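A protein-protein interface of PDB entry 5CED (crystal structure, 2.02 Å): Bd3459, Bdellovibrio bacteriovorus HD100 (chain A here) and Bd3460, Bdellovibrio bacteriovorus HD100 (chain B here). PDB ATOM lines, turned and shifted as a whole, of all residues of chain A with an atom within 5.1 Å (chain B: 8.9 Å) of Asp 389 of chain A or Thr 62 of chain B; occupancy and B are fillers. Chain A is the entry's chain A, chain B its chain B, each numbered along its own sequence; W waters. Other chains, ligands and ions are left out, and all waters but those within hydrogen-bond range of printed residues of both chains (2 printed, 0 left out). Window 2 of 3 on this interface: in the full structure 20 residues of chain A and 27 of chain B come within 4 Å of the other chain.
The backbone carbonyl oxygen (O) of Lys 390 of chain A sits at hydrogen-bond distance from the side-chain amide nitrogen (ND2) of Asn 94 of chain B.
The side-chain amide oxygen of Asn 362 of chain A is in hydrogen-bond range of the backbone NH of Asp 389 of chain A. NH1 of Arg 392 of chain A is in hydrogen-bond range of O of Asp 389 of chain A (2.7 Å). OD1 of Asp 60 of chain B lies within hydrogen-bond range of N of Thr 62 of chain B (2.9 Å). The side-chain carboxylate of Asp 60 of chain B sits at hydrogen-bond distance from the backbone NH of Met 64 of chain B (2.9 Å). The backbone carbonyl oxygen (O) of Thr 62 of chain B sits at hydrogen-bond distance from the backbone NH (N) of Asn 94 of chain B, at 2.9 Å. ND2 of Asn 93 of chain B sits at hydrogen-bond distance from OD1 of Asn 94 of chain B, 3.3 Å away.
Among the printed residues, merely in contact across the chains: Asp 389 of chain A with Thr 62 of chain B (3.7 Å), Lys 390 of chain A with Thr 62 of chain B (3.7 Å), Ser 391 of chain A with Asn 94 of chain B (3.999 Å), Arg 392 of chain A with Met 64 of chain B (3.8 Å), Arg 392 of chain A with Met 72 of chain B (3.96 Å) and Arg 392 of chain A with Phe 102 of chain B (3.9 Å).
Of chain B, only Thr 62 (3.7 Å) comes within 4 Å of Asp 389 of chain A. Of the printed residues of chain B, Lys 390 of chain A touches Thr 62 (3.7 Å) and Asn 94 (3.0 Å). Of chain A, only Asp 389 (3.7 Å) and Lys 390 (3.7 Å) come within 4 Å of Thr 62 of chain B. Printed residues of chain A within 4 Å of Phe 102 of chain B: Arg 392 (3.9 Å). The nearest residue of chain A that does not touch Thr 62 of chain B is Arg 392 of chain A (4.1 Å).
Of the 19 printed residues of chain B, 5 touch a printed residue of chain A. Of the 8 printed residues of chain A, 4 touch a printed residue of chain B. Printed residues of chain A that touch a printed residue of chain B: Asp 389, Lys 390, Ser 391 and Arg 392. Among the printed residues, no Asp or Glu carboxylate lies within 4 Å of a Lys or Arg side-chain nitrogen of the other chain.
Water W1 lies within hydrogen-bond range of OD1 of Asn 94 of chain B (2.8 Å), ND2 of Asn 93 of chain B (3.3 Å) and N of Arg 392 of chain A (3.3 Å). Water W2 lies within hydrogen-bond range of the side-chain hydroxyl (OG1) of Thr 62 of chain B, the side-chain amide oxygen (OD1) of Asn 94 of chain B, the side-chain amide nitrogen (ND2) of Asn 93 of chain B and the backbone NH (N) of Arg 392 of chain A.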
ATOM      1  N   ASN A 362       4.056   9.648  -0.492  1.00  0.00           N
ATOM      2  CA  ASN A 362       5.390   9.758  -1.037  1.00  0.00           C
ATOM      3  C   ASN A 362       6.454   9.354  -0.003  1.00  0.00           C
ATOM      4  O   ASN A 362       7.287   8.450  -0.235  1.00  0.00           O
ATOM      5  CB  ASN A 362       5.603  11.153  -1.557  1.00  0.00           C
ATOM      6  CG  ASN A 362       7.005  11.375  -2.061  1.00  0.00           C
ATOM      7  OD1 ASN A 362       7.721  10.432  -2.489  1.00  0.00           O
ATOM      8  ND2 ASN A 362       7.418  12.629  -2.015  1.00  0.00           N
ATOM      9  N   LYS A 363       6.358   9.953   1.164  1.00  0.00           N
ATOM     10  CA  LYS A 363       7.357   9.766   2.202  1.00  0.00           C
ATOM     11  C   LYS A 363       7.015   8.740   3.279  1.00  0.00           C
ATOM     12  O   LYS A 363       7.798   8.542   4.202  1.00  0.00           O
ATOM     13  CB  LYS A 363       7.745  11.135   2.828  1.00  0.00           C
ATOM     14  CG  LYS A 363       8.368  12.095   1.797  1.00  0.00           C
ATOM     15  CD  LYS A 363       9.607  11.496   1.103  1.00  0.00           C
ATOM     16  CE  LYS A 363      10.464  12.575   0.418  1.00  0.00           C
ATOM     17  NZ  LYS A 363      11.470  11.954  -0.506  1.00  0.00           N
ATOM     18  N   ASP A 387      10.846   6.814  -0.052  1.00  0.00           N
ATOM     19  CA  ASP A 387      11.067   7.914  -1.011  1.00  0.00           C
ATOM     20  C   ASP A 387      10.487   7.515  -2.367  1.00  0.00           C
ATOM     21  O   ASP A 387      11.204   7.365  -3.376  1.00  0.00           O
ATOM     22  CB  ASP A 387      12.542   8.311  -1.147  1.00  0.00           C
ATOM     23  CG  ASP A 387      13.156   8.769   0.173  1.00  0.00           C
ATOM     24  OD1 ASP A 387      12.961   9.942   0.641  1.00  0.00           O
ATOM     25  OD2 ASP A 387      13.876   7.911   0.745  1.00  0.00           O
ATOM     26  N   TYR A 388       9.178   7.388  -2.373  1.00  0.00           N
ATOM     27  CA  TYR A 388       8.463   6.887  -3.524  1.00  0.00           C
ATOM     28  C   TYR A 388       8.698   7.739  -4.774  1.00  0.00           C
ATOM     29  O   TYR A 388       8.796   7.172  -5.895  1.00  0.00           O
ATOM     30  CB  TYR A 388       7.011   6.657  -3.140  1.00  0.00           C
ATOM     31  CG  TYR A 388       5.933   6.796  -4.212  1.00  0.00           C
ATOM     32  CD1 TYR A 388       5.619   8.036  -4.709  1.00  0.00           C
ATOM     33  CD2 TYR A 388       5.152   5.712  -4.605  1.00  0.00           C
ATOM     34  CE1 TYR A 388       4.616   8.213  -5.623  1.00  0.00           C
ATOM     35  CE2 TYR A 388       4.116   5.889  -5.526  1.00  0.00           C
ATOM     36  CZ  TYR A 388       3.865   7.157  -6.015  1.00  0.00           C
ATOM     37  OH  TYR A 388       2.885   7.441  -6.940  1.00  0.00           O
ATOM     38  N   ASP A 389       8.913   9.057  -4.574  1.00  0.00           N
ATOM     39  CA  ASP A 389       9.340   9.965  -5.665  1.00  0.00           C
ATOM     40  C   ASP A 389      10.562   9.500  -6.398  1.00  0.00           C
ATOM     41  O   ASP A 389      10.603   9.564  -7.606  1.00  0.00           O
ATOM     42  CB  ASP A 389       9.553  11.476  -5.264  1.00  0.00           C
ATOM     43  CG  ASP A 389      10.346  11.715  -3.888  1.00  0.00           C
ATOM     44  OD1 ASP A 389      10.491  10.830  -2.982  1.00  0.00           O
ATOM     45  OD2 ASP A 389      10.739  12.889  -3.689  1.00  0.00           O
ATOM     46  N   LYS A 390      11.561   9.056  -5.665  1.00  0.00           N
ATOM     47  CA  LYS A 390      12.834   8.635  -6.234  1.00  0.00           C
ATOM     48  C   LYS A 390      12.836   7.144  -6.614  1.00  0.00           C
ATOM     49  O   LYS A 390      13.549   6.773  -7.501  1.00  0.00           O
ATOM     50  CB  LYS A 390      13.946   8.882  -5.211  1.00  0.00           C
ATOM     51  CG  LYS A 390      14.179  10.362  -4.895  1.00  0.00           C
ATOM     52  CD  LYS A 390      15.289  10.951  -5.751  1.00  0.00           C
ATOM     53  CE  LYS A 390      15.221  12.471  -5.903  1.00  0.00           C
ATOM     54  NZ  LYS A 390      14.844  13.146  -4.637  1.00  0.00           N
ATOM     55  N   SER A 391      12.071   6.297  -5.900  1.00  0.00           N
ATOM     56  CA  SER A 391      12.022   4.846  -6.197  1.00  0.00           C
ATOM     57  C   SER A 391      10.660   4.382  -5.890  1.00  0.00           C
ATOM     58  O   SER A 391      10.323   4.206  -4.728  1.00  0.00           O
ATOM     59  CB  SER A 391      13.022   4.007  -5.360  1.00  0.00           C
ATOM     60  OG  SER A 391      13.349   4.672  -4.163  1.00  0.00           O
ATOM     61  N   ARG A 392       9.874   4.202  -6.938  1.00  0.00           N
ATOM     62  CA  ARG A 392       8.459   3.781  -6.791  1.00  0.00           C
ATOM     63  C   ARG A 392       8.347   2.402  -6.179  1.00  0.00           C
ATOM     64  O   ARG A 392       7.300   2.072  -5.582  1.00  0.00           O
ATOM     65  CB  ARG A 392       7.748   3.852  -8.145  1.00  0.00           C
ATOM     66  CG  ARG A 392       7.668   5.263  -8.744  1.00  0.00           C
ATOM     67  CD  ARG A 392       6.671   6.107  -7.993  1.00  0.00           C
ATOM     68  NE  ARG A 392       6.332   7.301  -8.745  1.00  0.00           N
ATOM     69  CZ  ARG A 392       7.101   8.378  -8.922  1.00  0.00           C
ATOM     70  NH1 ARG A 392       8.301   8.480  -8.370  1.00  0.00           N
ATOM     71  NH2 ARG A 392       6.643   9.383  -9.654  1.00  0.00           N
ATOM     72  N   SER B  29       7.950   9.962 -22.775  1.00  0.00           N
ATOM     73  CA  SER B  29       6.983   9.647 -21.714  1.00  0.00           C
ATOM     74  C   SER B  29       6.137  10.886 -21.356  1.00  0.00           C
ATOM     75  O   SER B  29       6.569  12.026 -21.519  1.00  0.00           O
ATOM     76  CB  SER B  29       7.665   9.042 -20.469  1.00  0.00           C
ATOM     77  OG  SER B  29       8.501   9.968 -19.800  1.00  0.00           O
ATOM     78  N   ASN B  34       1.111   8.849 -16.917  1.00  0.00           N
ATOM     79  CA  ASN B  34       1.586   8.007 -15.823  1.00  0.00           C
ATOM     80  C   ASN B  34       0.804   8.271 -14.522  1.00  0.00           C
ATOM     81  O   ASN B  34       0.414   7.317 -13.802  1.00  0.00           O
ATOM     82  CB  ASN B  34       3.079   8.207 -15.615  1.00  0.00           C
ATOM     83  CG  ASN B  34       3.935   7.581 -16.727  1.00  0.00           C
ATOM     84  OD1 ASN B  34       3.477   6.785 -17.544  1.00  0.00           O
ATOM     85  ND2 ASN B  34       5.189   7.933 -16.735  1.00  0.00           N
ATOM     86  N   GLN B  59       9.949   5.074 -20.905  1.00  0.00           N
ATOM     87  CA  GLN B  59      10.105   5.049 -19.477  1.00  0.00           C
ATOM     88  C   GLN B  59      10.485   6.433 -19.008  1.00  0.00           C
ATOM     89  O   GLN B  59      11.263   7.128 -19.674  1.00  0.00           O
ATOM     90  CB  GLN B  59      11.196   4.055 -19.109  1.00  0.00           C
ATOM     91  CG  GLN B  59      10.746   2.620 -19.307  1.00  0.00           C
ATOM     92  CD  GLN B  59      11.875   1.615 -19.243  1.00  0.00           C
ATOM     93  OE1 GLN B  59      12.545   1.319 -20.254  1.00  0.00           O
ATOM     94  NE2 GLN B  59      12.078   1.073 -18.071  1.00  0.00           N
ATOM     95  N   ASP B  60       9.950   6.834 -17.865  1.00  0.00           N
ATOM     96  CA  ASP B  60      10.268   8.147 -17.304  1.00  0.00           C
ATOM     97  C   ASP B  60      11.600   8.137 -16.559  1.00  0.00           C
ATOM     98  O   ASP B  60      12.394   7.201 -16.660  1.00  0.00           O
ATOM     99  CB  ASP B  60       9.098   8.670 -16.423  1.00  0.00           C
ATOM    100  CG  ASP B  60       8.981   7.943 -15.047  1.00  0.00           C
ATOM    101  OD1 ASP B  60       9.869   7.139 -14.633  1.00  0.00           O
ATOM    102  OD2 ASP B  60       7.962   8.174 -14.363  1.00  0.00           O
ATOM    103  N   GLU B  61      11.808   9.182 -15.779  1.00  0.00           N
ATOM    104  CA  GLU B  61      13.035   9.473 -15.074  1.00  0.00           C
ATOM    105  C   GLU B  61      13.452   8.372 -14.067  1.00  0.00           C
ATOM    106  O   GLU B  61      14.661   8.161 -13.847  1.00  0.00           O
ATOM    107  CB  GLU B  61      12.858  10.835 -14.345  1.00  0.00           C
ATOM    108  CG  GLU B  61      12.515  12.020 -15.296  1.00  0.00           C
ATOM    109  CD  GLU B  61      11.031  12.151 -15.785  1.00  0.00           C
ATOM    110  OE1 GLU B  61      10.103  11.732 -15.075  1.00  0.00           O
ATOM    111  OE2 GLU B  61      10.799  12.700 -16.899  1.00  0.00           O
ATOM    112  N   THR B  62      12.476   7.682 -13.462  1.00  0.00           N
ATOM    113  CA  THR B  62      12.784   6.582 -12.552  1.00  0.00           C
ATOM    114  C   THR B  62      12.543   5.208 -13.215  1.00  0.00           C
ATOM    115  O   THR B  62      12.521   4.192 -12.541  1.00  0.00           O
ATOM    116  CB  THR B  62      12.042   6.724 -11.196  1.00  0.00           C
ATOM    117  OG1 THR B  62      10.678   6.304 -11.317  1.00  0.00           O
ATOM    118  CG2 THR B  62      12.123   8.194 -10.646  1.00  0.00           C
ATOM    119  N   GLY B  63      12.411   5.195 -14.541  1.00  0.00           N
ATOM    120  CA  GLY B  63      12.194   3.982 -15.304  1.00  0.00           C
ATOM    121  C   GLY B  63      10.761   3.492 -15.380  1.00  0.00           C
ATOM    122  O   GLY B  63      10.530   2.369 -15.805  1.00  0.00           O
ATOM    123  N   MET B  64       9.794   4.309 -14.964  1.00  0.00           N
ATOM    124  CA  MET B  64       8.384   3.845 -14.932  1.00  0.00           C
ATOM    125  C   MET B  64       7.697   3.985 -16.293  1.00  0.00           C
ATOM    126  O   MET B  64       7.859   4.996 -16.972  1.00  0.00           O
ATOM    127  CB  MET B  64       7.548   4.667 -13.944  1.00  0.00           C
ATOM    128  CG  MET B  64       8.008   4.562 -12.494  1.00  0.00           C
ATOM    129  SD  MET B  64       7.716   2.920 -11.807  1.00  0.00           S
ATOM    130  CE  MET B  64       5.945   3.070 -11.444  1.00  0.00           C
ATOM    131  N   THR B  65       6.890   2.974 -16.622  1.00  0.00           N
ATOM    132  CA  THR B  65       5.924   3.018 -17.687  1.00  0.00           C
ATOM    133  C   THR B  65       4.468   3.243 -17.230  1.00  0.00           C
ATOM    134  O   THR B  65       4.116   3.021 -16.051  1.00  0.00           O
ATOM    135  CB  THR B  65       5.928   1.690 -18.432  1.00  0.00           C
ATOM    136  OG1 THR B  65       5.550   0.608 -17.561  1.00  0.00           O
ATOM    137  CG2 THR B  65       7.292   1.470 -19.064  1.00  0.00           C
ATOM    138  N   MET B  68       3.315   0.004 -15.507  1.00  0.00           N
ATOM    139  CA  MET B  68       3.796  -0.148 -14.145  1.00  0.00           C
ATOM    140  C   MET B  68       2.981   0.711 -13.184  1.00  0.00           C
ATOM    141  O   MET B  68       2.644   0.262 -12.065  1.00  0.00           O
ATOM    142  CB  MET B  68       5.267   0.212 -13.983  1.00  0.00           C
ATOM    143  CG  MET B  68       6.289  -0.672 -14.679  1.00  0.00           C
ATOM    144  SD  MET B  68       7.898   0.220 -14.674  1.00  0.00           S
ATOM    145  CE  MET B  68       8.630  -0.619 -16.058  1.00  0.00           C
ATOM    146  N   ASN B  69       2.678   1.926 -13.602  1.00  0.00           N
ATOM    147  CA  ASN B  69       1.788   2.777 -12.832  1.00  0.00           C
ATOM    148  C   ASN B  69       0.399   2.169 -12.606  1.00  0.00           C
ATOM    149  O   ASN B  69      -0.113   2.162 -11.474  1.00  0.00           O
ATOM    150  CB  ASN B  69       1.662   4.125 -13.507  1.00  0.00           C
ATOM    151  CG  ASN B  69       2.793   5.054 -13.140  1.00  0.00           C
ATOM    152  OD1 ASN B  69       2.771   5.613 -12.052  1.00  0.00           O
ATOM    153  ND2 ASN B  69       3.791   5.203 -14.013  1.00  0.00           N
ATOM    154  N   MET B  72       0.749  -0.957 -10.205  1.00  0.00           N
ATOM    155  CA  MET B  72       1.004  -0.495  -8.849  1.00  0.00           C
ATOM    156  C   MET B  72      -0.262  -0.010  -8.184  1.00  0.00           C
ATOM    157  O   MET B  72      -0.501  -0.286  -7.014  1.00  0.00           O
ATOM    158  CB  MET B  72       2.006   0.661  -8.869  1.00  0.00           C
ATOM    159  CG  MET B  72       2.235   1.300  -7.523  1.00  0.00           C
ATOM    160  SD  MET B  72       3.831   2.133  -7.491  1.00  0.00           S
ATOM    161  CE  MET B  72       3.585   3.254  -8.843  1.00  0.00           C
ATOM    162  N   LYS B  92      11.617  -2.675 -16.889  1.00  0.00           N
ATOM    163  CA  LYS B  92      11.903  -2.601 -15.457  1.00  0.00           C
ATOM    164  C   LYS B  92      12.188  -1.157 -15.049  1.00  0.00           C
ATOM    165  O   LYS B  92      12.857  -0.451 -15.788  1.00  0.00           O
ATOM    166  CB  LYS B  92      13.115  -3.465 -15.090  1.00  0.00           C
ATOM    167  CG  LYS B  92      12.868  -4.957 -15.279  1.00  0.00           C
ATOM    168  CD  LYS B  92      14.195  -5.735 -15.171  1.00  0.00           C
ATOM    169  CE  LYS B  92      13.967  -7.236 -15.344  1.00  0.00           C
ATOM    170  NZ  LYS B  92      15.203  -8.040 -15.634  1.00  0.00           N
ATOM    171  N   ASN B  93      11.682  -0.738 -13.888  1.00  0.00           N
ATOM    172  CA  ASN B  93      12.070   0.561 -13.316  1.00  0.00           C
ATOM    173  C   ASN B  93      13.449   0.538 -12.673  1.00  0.00           C
ATOM    174  O   ASN B  93      14.166  -0.496 -12.721  1.00  0.00           O
ATOM    175  CB  ASN B  93      11.027   1.017 -12.328  1.00  0.00           C
ATOM    176  CG  ASN B  93      11.146   0.325 -10.981  1.00  0.00           C
ATOM    177  OD1 ASN B  93      11.505  -0.858 -10.892  1.00  0.00           O
ATOM    178  ND2 ASN B  93      10.898   1.073  -9.925  1.00  0.00           N
ATOM    179  N   ASN B  94      13.832   1.640 -12.040  1.00  0.00           N
ATOM    180  CA  ASN B  94      15.109   1.677 -11.323  1.00  0.00           C
ATOM    181  C   ASN B  94      15.235   0.666 -10.164  1.00  0.00           C
ATOM    182  O   ASN B  94      16.351   0.298  -9.788  1.00  0.00           O
ATOM    183  CB  ASN B  94      15.484   3.136 -10.893  1.00  0.00           C
ATOM    184  CG  ASN B  94      14.530   3.710  -9.844  1.00  0.00           C
ATOM    185  OD1 ASN B  94      13.543   3.062  -9.437  1.00  0.00           O
ATOM    186  ND2 ASN B  94      14.789   4.906  -9.432  1.00  0.00           N
ATOM    187  N   GLY B  95      14.131   0.194  -9.581  1.00  0.00           N
ATOM    188  CA  GLY B  95      14.232  -0.850  -8.550  1.00  0.00           C
ATOM    189  C   GLY B  95      14.295  -2.244  -9.168  1.00  0.00           C
ATOM    190  O   GLY B  95      14.232  -3.229  -8.435  1.00  0.00           O
ATOM    191  N   GLY B  96      14.366  -2.334 -10.511  1.00  0.00           N
ATOM    192  CA  GLY B  96      14.496  -3.614 -11.230  1.00  0.00           C
ATOM    193  C   GLY B  96      13.190  -4.401 -11.387  1.00  0.00           C
ATOM    194  O   GLY B  96      13.218  -5.603 -11.640  1.00  0.00           O
ATOM    195  N   GLU B  97      12.045  -3.718 -11.223  1.00  0.00           N
ATOM    196  CA  GLU B  97      10.747  -4.350 -11.123  1.00  0.00           C
ATOM    197  C   GLU B  97       9.954  -4.155 -12.428  1.00  0.00           C
ATOM    198  O   GLU B  97       9.913  -3.066 -12.995  1.00  0.00           O
ATOM    199  CB  GLU B  97       9.952  -3.784  -9.938  1.00  0.00           C
ATOM    200  CG  GLU B  97      10.460  -4.315  -8.580  1.00  0.00           C
ATOM    201  CD  GLU B  97       9.579  -3.912  -7.409  1.00  0.00           C
ATOM    202  OE1 GLU B  97       9.042  -2.782  -7.451  1.00  0.00           O
ATOM    203  OE2 GLU B  97       9.389  -4.755  -6.471  1.00  0.00           O
ATOM    204  N   PHE B 102       5.356  -5.044  -9.638  1.00  0.00           N
ATOM    205  CA  PHE B 102       4.604  -3.933  -8.979  1.00  0.00           C
ATOM    206  C   PHE B 102       3.254  -4.423  -8.467  1.00  0.00           C
ATOM    207  O   PHE B 102       2.865  -4.107  -7.328  1.00  0.00           O
ATOM    208  CB  PHE B 102       4.395  -2.711  -9.889  1.00  0.00           C
ATOM    209  CG  PHE B 102       5.544  -1.779  -9.910  1.00  0.00           C
ATOM    210  CD1 PHE B 102       5.688  -0.813  -8.914  1.00  0.00           C
ATOM    211  CD2 PHE B 102       6.484  -1.831 -10.919  1.00  0.00           C
ATOM    212  CE1 PHE B 102       6.754   0.051  -8.899  1.00  0.00           C
ATOM    213  CE2 PHE B 102       7.563  -0.945 -10.920  1.00  0.00           C
ATOM    214  CZ  PHE B 102       7.724  -0.038  -9.906  1.00  0.00           C
HETATM  215  O   HOH W   1      12.331   2.029  -7.163  1.00  0.00           O
HETATM  216  O   HOH W   2      10.780   4.004  -9.736  1.00  0.00           O
